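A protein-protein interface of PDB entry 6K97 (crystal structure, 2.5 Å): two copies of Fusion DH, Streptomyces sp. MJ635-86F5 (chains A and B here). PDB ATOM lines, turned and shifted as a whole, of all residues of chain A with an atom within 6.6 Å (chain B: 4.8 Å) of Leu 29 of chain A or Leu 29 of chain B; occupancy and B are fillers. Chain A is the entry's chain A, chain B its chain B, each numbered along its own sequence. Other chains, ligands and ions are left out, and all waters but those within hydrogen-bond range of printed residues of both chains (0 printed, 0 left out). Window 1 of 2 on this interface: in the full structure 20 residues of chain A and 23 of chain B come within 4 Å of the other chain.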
ATOM      1  N   ALA A  24     -10.015 -17.433   0.138  1.00  0.00           N
ATOM      2  CA  ALA A  24      -8.532 -17.058   0.129  1.00  0.00           C
ATOM      3  C   ALA A  24      -7.995 -16.767  -1.265  1.00  0.00           C
ATOM      4  O   ALA A  24      -7.481 -15.683  -1.527  1.00  0.00           O
ATOM      5  CB  ALA A  24      -7.658 -18.089   0.799  1.00  0.00           C
ATOM      6  N   ALA A  25      -8.086 -17.736  -2.150  1.00  0.00           N
ATOM      7  CA  ALA A  25      -7.923 -17.454  -3.539  1.00  0.00           C
ATOM      8  C   ALA A  25      -8.851 -16.262  -3.939  1.00  0.00           C
ATOM      9  O   ALA A  25      -8.475 -15.457  -4.770  1.00  0.00           O
ATOM     10  CB  ALA A  25      -8.249 -18.676  -4.368  1.00  0.00           C
ATOM     11  N   GLY A  26     -10.056 -16.173  -3.375  1.00  0.00           N
ATOM     12  CA  GLY A  26     -11.026 -15.142  -3.793  1.00  0.00           C
ATOM     13  C   GLY A  26     -10.520 -13.758  -3.492  1.00  0.00           C
ATOM     14  O   GLY A  26     -10.969 -12.792  -4.109  1.00  0.00           O
ATOM     15  N   LEU A  27      -9.568 -13.652  -2.541  1.00  0.00           N
ATOM     16  CA  LEU A  27      -8.977 -12.378  -2.217  1.00  0.00           C
ATOM     17  C   LEU A  27      -7.576 -12.135  -2.816  1.00  0.00           C
ATOM     18  O   LEU A  27      -6.977 -11.071  -2.629  1.00  0.00           O
ATOM     19  CB  LEU A  27      -8.964 -12.187  -0.699  1.00  0.00           C
ATOM     20  CG  LEU A  27     -10.347 -12.206   0.011  1.00  0.00           C
ATOM     21  CD1 LEU A  27     -10.105 -12.227   1.510  1.00  0.00           C
ATOM     22  CD2 LEU A  27     -11.273 -11.051  -0.334  1.00  0.00           C
ATOM     23  N   GLY A  28      -7.088 -13.110  -3.579  1.00  0.00           N
ATOM     24  CA  GLY A  28      -5.783 -13.020  -4.200  1.00  0.00           C
ATOM     25  C   GLY A  28      -4.674 -13.632  -3.381  1.00  0.00           C
ATOM     26  O   GLY A  28      -3.538 -13.355  -3.671  1.00  0.00           O
ATOM     27  N   LEU A  29      -4.981 -14.425  -2.349  1.00  0.00           N
ATOM     28  CA  LEU A  29      -3.950 -15.055  -1.469  1.00  0.00           C
ATOM     29  C   LEU A  29      -3.885 -16.570  -1.525  1.00  0.00           C
ATOM     30  O   LEU A  29      -4.827 -17.223  -1.888  1.00  0.00           O
ATOM     31  CB  LEU A  29      -4.208 -14.690  -0.010  1.00  0.00           C
ATOM     32  CG  LEU A  29      -4.126 -13.191   0.241  1.00  0.00           C
ATOM     33  CD1 LEU A  29      -5.417 -12.681   0.894  1.00  0.00           C
ATOM     34  CD2 LEU A  29      -2.908 -12.830   1.087  1.00  0.00           C
ATOM     35  N   GLU A  30      -2.770 -17.111  -1.083  1.00  0.00           N
ATOM     36  CA  GLU A  30      -2.551 -18.550  -0.997  1.00  0.00           C
ATOM     37  C   GLU A  30      -2.928 -18.994   0.405  1.00  0.00           C
ATOM     38  O   GLU A  30      -2.543 -18.350   1.385  1.00  0.00           O
ATOM     39  CB  GLU A  30      -1.070 -18.892  -1.325  1.00  0.00           C
ATOM     40  CG  GLU A  30      -0.684 -18.547  -2.766  1.00  0.00           C
ATOM     41  CD  GLU A  30       0.737 -17.994  -2.986  1.00  0.00           C
ATOM     42  OE1 GLU A  30       1.260 -17.142  -2.208  1.00  0.00           O
ATOM     43  OE2 GLU A  30       1.342 -18.400  -3.994  1.00  0.00           O
ATOM     44  N   ALA A  31      -3.668 -20.099   0.507  1.00  0.00           N
ATOM     45  CA  ALA A  31      -4.093 -20.640   1.789  1.00  0.00           C
ATOM     46  C   ALA A  31      -2.949 -21.387   2.450  1.00  0.00           C
ATOM     47  O   ALA A  31      -1.978 -21.762   1.772  1.00  0.00           O
ATOM     48  CB  ALA A  31      -5.275 -21.566   1.610  1.00  0.00           C
ATOM     49  N   THR A  39      -3.932 -17.951   5.760  1.00  0.00           N
ATOM     50  CA  THR A  39      -3.143 -17.630   4.555  1.00  0.00           C
ATOM     51  C   THR A  39      -1.617 -17.666   4.775  1.00  0.00           C
ATOM     52  O   THR A  39      -1.134 -17.518   5.886  1.00  0.00           O
ATOM     53  CB  THR A  39      -3.463 -16.199   4.011  1.00  0.00           C
ATOM     54  OG1 THR A  39      -2.925 -15.205   4.899  1.00  0.00           O
ATOM     55  CG2 THR A  39      -4.961 -15.964   3.827  1.00  0.00           C
ATOM     56  N   ALA A  40      -0.873 -17.802   3.674  1.00  0.00           N
ATOM     57  CA  ALA A  40       0.606 -17.706   3.641  1.00  0.00           C
ATOM     58  C   ALA A  40       1.058 -17.159   2.324  1.00  0.00           C
ATOM     59  O   ALA A  40       0.662 -17.675   1.328  1.00  0.00           O
ATOM     60  CB  ALA A  40       1.202 -19.082   3.801  1.00  0.00           C
ATOM     61  N   THR A  41       1.867 -16.113   2.272  1.00  0.00           N
ATOM     62  CA  THR A  41       2.323 -15.662   0.998  1.00  0.00           C
ATOM     63  C   THR A  41       3.763 -15.287   1.061  1.00  0.00           C
ATOM     64  O   THR A  41       4.214 -14.751   2.061  1.00  0.00           O
ATOM     65  CB  THR A  41       1.503 -14.472   0.459  1.00  0.00           C
ATOM     66  OG1 THR A  41       2.188 -13.257   0.727  1.00  0.00           O
ATOM     67  CG2 THR A  41       0.150 -14.367   1.082  1.00  0.00           C
ATOM     68  N   LEU A  49       4.227 -13.521   4.735  1.00  0.00           N
ATOM     69  CA  LEU A  49       3.134 -12.977   5.565  1.00  0.00           C
ATOM     70  C   LEU A  49       2.153 -14.117   5.834  1.00  0.00           C
ATOM     71  O   LEU A  49       1.756 -14.806   4.897  1.00  0.00           O
ATOM     72  CB  LEU A  49       2.407 -11.832   4.861  1.00  0.00           C
ATOM     73  CG  LEU A  49       1.198 -11.269   5.637  1.00  0.00           C
ATOM     74  CD1 LEU A  49       1.632 -10.484   6.884  1.00  0.00           C
ATOM     75  CD2 LEU A  49       0.296 -10.379   4.795  1.00  0.00           C
ATOM     76  N   THR A  51      -1.682 -14.846   7.817  1.00  0.00           N
ATOM     77  CA  THR A  51      -2.789 -14.125   8.459  1.00  0.00           C
ATOM     78  C   THR A  51      -3.873 -15.067   8.924  1.00  0.00           C
ATOM     79  O   THR A  51      -4.043 -16.166   8.374  1.00  0.00           O
ATOM     80  CB  THR A  51      -3.457 -13.075   7.529  1.00  0.00           C
ATOM     81  OG1 THR A  51      -4.278 -13.726   6.531  1.00  0.00           O
ATOM     82  CG2 THR A  51      -2.411 -12.233   6.824  1.00  0.00           C
ATOM     83  N   GLY A  52      -4.615 -14.625   9.934  1.00  0.00           N
ATOM     84  CA  GLY A  52      -5.779 -15.370  10.401  1.00  0.00           C
ATOM     85  C   GLY A  52      -6.648 -14.518  11.279  1.00  0.00           C
ATOM     86  O   GLY A  52      -6.242 -13.447  11.744  1.00  0.00           O
ATOM     87  N   ARG A  53      -7.857 -15.004  11.500  1.00  0.00           N
ATOM     88  CA  ARG A  53      -8.819 -14.348  12.374  1.00  0.00           C
ATOM     89  C   ARG A  53      -8.772 -15.083  13.699  1.00  0.00           C
ATOM     90  O   ARG A  53      -8.803 -16.315  13.728  1.00  0.00           O
ATOM     91  CB  ARG A  53     -10.235 -14.434  11.784  1.00  0.00           C
ATOM     92  CG  ARG A  53     -11.286 -13.690  12.600  1.00  0.00           C
ATOM     93  CD  ARG A  53     -12.651 -13.705  11.921  1.00  0.00           C
ATOM     94  NE  ARG A  53     -13.612 -12.897  12.675  1.00  0.00           N
ATOM     95  CZ  ARG A  53     -14.416 -13.361  13.640  1.00  0.00           C
ATOM     96  NH1 ARG A  53     -14.415 -14.653  13.980  1.00  0.00           N
ATOM     97  NH2 ARG A  53     -15.244 -12.537  14.270  1.00  0.00           N
ATOM     98  N   LEU A 112      -7.709  -9.517  14.100  1.00  0.00           N
ATOM     99  CA  LEU A 112      -6.878  -9.906  12.976  1.00  0.00           C
ATOM    100  C   LEU A 112      -5.498 -10.263  13.511  1.00  0.00           C
ATOM    101  O   LEU A 112      -4.901  -9.489  14.199  1.00  0.00           O
ATOM    102  CB  LEU A 112      -6.772  -8.804  11.943  1.00  0.00           C
ATOM    103  CG  LEU A 112      -8.077  -8.197  11.430  1.00  0.00           C
ATOM    104  CD1 LEU A 112      -7.750  -7.392  10.194  1.00  0.00           C
ATOM    105  CD2 LEU A 112      -9.142  -9.251  11.127  1.00  0.00           C
ATOM    106  N   LEU A 113      -5.004 -11.430  13.165  1.00  0.00           N
ATOM    107  CA  LEU A 113      -3.707 -11.946  13.609  1.00  0.00           C
ATOM    108  C   LEU A 113      -2.745 -12.111  12.420  1.00  0.00           C
ATOM    109  O   LEU A 113      -3.100 -12.685  11.361  1.00  0.00           O
ATOM    110  CB  LEU A 113      -3.938 -13.318  14.231  1.00  0.00           C
ATOM    111  CG  LEU A 113      -2.693 -13.949  14.794  1.00  0.00           C
ATOM    112  CD1 LEU A 113      -2.114 -13.132  15.945  1.00  0.00           C
ATOM    113  CD2 LEU A 113      -3.008 -15.391  15.230  1.00  0.00           C
ATOM    114  N   GLN A 114      -1.519 -11.672  12.615  1.00  0.00           N
ATOM    115  CA  GLN A 114      -0.501 -11.661  11.550  1.00  0.00           C
ATOM    116  C   GLN A 114       0.876 -12.084  12.061  1.00  0.00           C
ATOM    117  O   GLN A 114       1.309 -11.676  13.139  1.00  0.00           O
ATOM    118  CB  GLN A 114      -0.407 -10.307  10.870  1.00  0.00           C
ATOM    119  CG  GLN A 114      -1.693 -10.051  10.082  1.00  0.00           C
ATOM    120  CD  GLN A 114      -1.671  -8.887   9.089  1.00  0.00           C
ATOM    121  OE1 GLN A 114      -0.752  -8.024   9.077  1.00  0.00           O
ATOM    122  NE2 GLN A 114      -2.715  -8.853   8.249  1.00  0.00           N
ATOM    123  N   TRP A 140      -1.889  -1.681  15.060  1.00  0.00           N
ATOM    124  CA  TRP A 140      -1.337  -2.983  15.328  1.00  0.00           C
ATOM    125  C   TRP A 140      -0.695  -2.989  16.676  1.00  0.00           C
ATOM    126  O   TRP A 140      -0.115  -2.007  17.041  1.00  0.00           O
ATOM    127  CB  TRP A 140      -0.274  -3.334  14.304  1.00  0.00           C
ATOM    128  CG  TRP A 140      -0.818  -3.577  12.964  1.00  0.00           C
ATOM    129  CD1 TRP A 140      -0.726  -2.744  11.872  1.00  0.00           C
ATOM    130  CD2 TRP A 140      -1.560  -4.720  12.540  1.00  0.00           C
ATOM    131  NE1 TRP A 140      -1.339  -3.327  10.788  1.00  0.00           N
ATOM    132  CE2 TRP A 140      -1.862  -4.534  11.166  1.00  0.00           C
ATOM    133  CE3 TRP A 140      -1.994  -5.883  13.180  1.00  0.00           C
ATOM    134  CZ2 TRP A 140      -2.608  -5.444  10.437  1.00  0.00           C
ATOM    135  CZ3 TRP A 140      -2.712  -6.817  12.447  1.00  0.00           C
ATOM    136  CH2 TRP A 140      -3.012  -6.585  11.066  1.00  0.00           C
ATOM    137  N   ALA B  24     -12.550 -10.898   4.076  1.00  0.00           N
ATOM    138  CA  ALA B  24     -11.182 -10.263   4.278  1.00  0.00           C
ATOM    139  C   ALA B  24     -10.749 -10.209   5.747  1.00  0.00           C
ATOM    140  O   ALA B  24      -9.726 -10.761   6.113  1.00  0.00           O
ATOM    141  CB  ALA B  24     -11.080  -8.886   3.667  1.00  0.00           C
ATOM    142  N   ALA B  25     -11.524  -9.531   6.567  1.00  0.00           N
ATOM    143  CA  ALA B  25     -11.411  -9.662   7.990  1.00  0.00           C
ATOM    144  C   ALA B  25     -11.459 -11.134   8.390  1.00  0.00           C
ATOM    145  O   ALA B  25     -10.776 -11.535   9.322  1.00  0.00           O
ATOM    146  CB  ALA B  25     -12.526  -8.890   8.684  1.00  0.00           C
ATOM    147  N   LEU B  27     -10.207 -13.693   6.943  1.00  0.00           N
ATOM    148  CA  LEU B  27      -8.915 -14.328   6.765  1.00  0.00           C
ATOM    149  C   LEU B  27      -7.748 -13.656   7.532  1.00  0.00           C
ATOM    150  O   LEU B  27      -6.585 -14.099   7.435  1.00  0.00           O
ATOM    151  CB  LEU B  27      -8.585 -14.410   5.291  1.00  0.00           C
ATOM    152  CG  LEU B  27      -9.624 -15.205   4.495  1.00  0.00           C
ATOM    153  CD1 LEU B  27      -9.338 -14.987   3.011  1.00  0.00           C
ATOM    154  CD2 LEU B  27      -9.670 -16.683   4.801  1.00  0.00           C
ATOM    155  N   GLY B  28      -8.057 -12.619   8.309  1.00  0.00           N
ATOM    156  CA  GLY B  28      -7.039 -11.874   9.023  1.00  0.00           C
ATOM    157  C   GLY B  28      -6.446 -10.677   8.272  1.00  0.00           C
ATOM    158  O   GLY B  28      -5.413 -10.191   8.689  1.00  0.00           O
ATOM    159  N   LEU B  29      -7.090 -10.175   7.218  1.00  0.00           N
ATOM    160  CA  LEU B  29      -6.608  -8.993   6.453  1.00  0.00           C
ATOM    161  C   LEU B  29      -7.517  -7.771   6.465  1.00  0.00           C
ATOM    162  O   LEU B  29      -8.698  -7.878   6.714  1.00  0.00           O
ATOM    163  CB  LEU B  29      -6.406  -9.377   4.989  1.00  0.00           C
ATOM    164  CG  LEU B  29      -5.338 -10.479   4.819  1.00  0.00           C
ATOM    165  CD1 LEU B  29      -5.944 -11.649   4.083  1.00  0.00           C
ATOM    166  CD2 LEU B  29      -4.074  -9.955   4.155  1.00  0.00           C
ATOM    167  N   GLU B  30      -6.941  -6.619   6.153  1.00  0.00           N
ATOM    168  CA  GLU B  30      -7.656  -5.378   6.045  1.00  0.00           C
ATOM    169  C   GLU B  30      -8.077  -5.236   4.602  1.00  0.00           C
ATOM    170  O   GLU B  30      -7.272  -5.430   3.691  1.00  0.00           O
ATOM    171  CB  GLU B  30      -6.758  -4.199   6.496  1.00  0.00           C
ATOM    172  CG  GLU B  30      -6.411  -4.259   7.985  1.00  0.00           C
ATOM    173  CD  GLU B  30      -5.002  -3.761   8.368  1.00  0.00           C
ATOM    174  OE1 GLU B  30      -3.971  -4.071   7.697  1.00  0.00           O
ATOM    175  OE2 GLU B  30      -4.923  -3.062   9.412  1.00  0.00           O
ATOM    176  N   ALA B  31      -9.338  -4.866   4.385  1.00  0.00           N
ATOM    177  CA  ALA B  31      -9.866  -4.660   3.048  1.00  0.00           C
ATOM    178  C   ALA B  31      -9.405  -3.334   2.496  1.00  0.00           C
ATOM    179  O   ALA B  31      -8.983  -2.469   3.238  1.00  0.00           O
ATOM    180  CB  ALA B  31     -11.384  -4.715   3.078  1.00  0.00           C
ATOM    181  N   THR B  39      -7.589  -6.426  -0.775  1.00  0.00           N
ATOM    182  CA  THR B  39      -6.890  -6.226   0.518  1.00  0.00           C
ATOM    183  C   THR B  39      -5.730  -5.226   0.461  1.00  0.00           C
ATOM    184  O   THR B  39      -5.178  -4.964  -0.596  1.00  0.00           O
ATOM    185  CB  THR B  39      -6.270  -7.549   1.055  1.00  0.00           C
ATOM    186  OG1 THR B  39      -5.128  -7.908   0.260  1.00  0.00           O
ATOM    187  CG2 THR B  39      -7.258  -8.695   1.065  1.00  0.00           C
ATOM    188  N   THR B  41      -2.388  -4.215   3.338  1.00  0.00           N
ATOM    189  CA  THR B  41      -1.860  -4.291   4.643  1.00  0.00           C
ATOM    190  C   THR B  41      -0.519  -3.565   4.704  1.00  0.00           C
ATOM    191  O   THR B  41       0.263  -3.628   3.788  1.00  0.00           O
ATOM    192  CB  THR B  41      -1.716  -5.754   5.136  1.00  0.00           C
ATOM    193  OG1 THR B  41      -0.373  -6.155   4.982  1.00  0.00           O
ATOM    194  CG2 THR B  41      -2.657  -6.756   4.423  1.00  0.00           C
ATOM    195  N   THR B  51      -3.608  -7.292  -2.455  1.00  0.00           N
ATOM    196  CA  THR B  51      -3.930  -8.498  -3.210  1.00  0.00           C
ATOM    197  C   THR B  51      -5.307  -8.426  -3.836  1.00  0.00           C
ATOM    198  O   THR B  51      -6.213  -7.747  -3.330  1.00  0.00           O
ATOM    199  CB  THR B  51      -3.841  -9.734  -2.339  1.00  0.00           C
ATOM    200  OG1 THR B  51      -4.967  -9.787  -1.454  1.00  0.00           O
ATOM    201  CG2 THR B  51      -2.561  -9.722  -1.515  1.00  0.00           C
ATOM    202  N   LEU B 112      -4.021 -15.000  -9.154  1.00  0.00           N
ATOM    203  CA  LEU B 112      -3.801 -14.235  -7.951  1.00  0.00           C
ATOM    204  C   LEU B 112      -2.948 -13.034  -8.325  1.00  0.00           C
ATOM    205  O   LEU B 112      -1.897 -13.204  -8.879  1.00  0.00           O
ATOM    206  CB  LEU B 112      -3.078 -15.032  -6.882  1.00  0.00           C
ATOM    207  CG  LEU B 112      -3.694 -16.356  -6.477  1.00  0.00           C
ATOM    208  CD1 LEU B 112      -3.066 -16.762  -5.163  1.00  0.00           C
ATOM    209  CD2 LEU B 112      -5.208 -16.266  -6.333  1.00  0.00           C
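OG1 of Thr 51 of chain B is in hydrogen-bond range of O of Leu 27 of chain A, at 2.7 Å.
NE2 of Gln 114 of chain A lies within hydrogen-bond range of O of Gly 28 of chain B.
The side-chain hydroxyl (OG1) of Thr 51 of chain A sits at hydrogen-bond distance from the backbone carbonyl oxygen (O) of Leu 27 of chain B (2.5 Å).
The backbone NH (N) of Gly 52 of chain A sits at hydrogen-bond distance from the backbone carbonyl oxygen (O) of Leu 27 of chain B, at 3.2 Å.
N of Leu 29 of chain B is in hydrogen-bond range of O of Ala 24 of chain B, 2.9 Å away.
The backbone NH (N) of Ala 40 of chain A sits at hydrogen-bond distance from the backbone carbonyl oxygen (O) of Glu 30 of chain A, at 2.9 Å.
The backbone carbonyl oxygen (O) of Gly 52 of chain A is in hydrogen-bond range of the backbone NH (N) of Leu 113 of chain A (2.8 Å).
N of Leu 29 of chain A lies within hydrogen-bond range of O of Ala 24 of chain A (2.9 Å).
The side-chain hydroxyl (OG1) of Thr 39 of chain A lies within hydrogen-bond range of the side-chain hydroxyl (OG1) of Thr 51 of chain A, at 2.6 Å.
The side-chain hydroxyl of Thr 39 of chain B sits at hydrogen-bond distance from the side-chain hydroxyl of Thr 51 of chain B, 2.5 Å away.
O of Ala 25 of chain A touches CD2 of Leu 112 of chain B, 3.7 Å away.
Thr 51 of chain B touches Gly 28 of chain A.
Leu 29 of chain A touches Leu 112 of chain B.
Glu 30 of chain A touches Leu 112 of chain B.
O of Gly 28 of chain B touches CB of Thr 51 of chain A (3.7 Å).
Gly 28 of chain B touches Gly 52 of chain A.
O of Ala 25 of chain B touches CB of Arg 53 of chain A, 3.8 Å away.
Leu 112 of chain A touches Ala 25 of chain B (CD2 to O, 3.3 Å).
CB of Leu 112 of chain A touches O of Gly 28 of chain B (3.8 Å).
Leu 112 of chain A touches Leu 29 of chain B (CD1 to O, 3.6 Å).
Leu 29 of chain A touches three residues of chain B.
Of chain A, only Leu 29 (3.4 Å), Thr 51 (3.6 Å) and Leu 112 (3.6 Å) come within 4 Å of Leu 29 of chain B.
Of the printed residues of chain A, Leu 27 of chain B touches Ala 24 (3.6 Å), Leu 27 (3.2 Å), Thr 51 (2.5 Å) and Gly 52 (3.2 Å).
Of the printed residues of chain B, Leu 112 of chain A touches Ala 25, Gly 28 and Leu 29.
Leu 49 of chain A touches none of the printed residues of chain B.
Thr 41 of chain B touches none of the printed residues of chain A.
Of the 11 printed residues of chain B, 8 touch a printed residue of chain A.
Hydrophobic or aromatic side chains of chain B within 4 Å of the printed part of chain A: Leu 27, Leu 29 and Leu 112.
Hydrophobic or aromatic side chains of chain A within 4 Å of the printed part of chain B: Leu 27, Leu 29, Leu 112 and Trp 140.
Among the printed residues, 23 pairs touch across the chains.
Among the printed residues, no Asp or Glu carboxylate lies within 4 Å of a Lys or Arg side-chain nitrogen of the other chain.
Ala 25 of chain A touches Leu 112 of chain B, and with the chains exchanged Leu 112 of chain A touches Ala 25 of chain B.
Leu 27 of chain A touches its own counterpart, Leu 27 of chain B.
Leu 29 of chain A touches Thr 51 of chain B, and with the chains exchanged Thr 51 of chain A touches Leu 29 of chain B.
Leu 29 of chain A touches Leu 112 of chain B, and with the chains exchanged Leu 112 of chain A touches Leu 29 of chain B.
Positions printed for both chains: 24, 25, 27, 28, 29, 30, 31, 39, 41, 51 and 112.
Of the 23 pairs that touch across the chains among the printed residues, 16 have their exchanged pair printed and touching as well.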
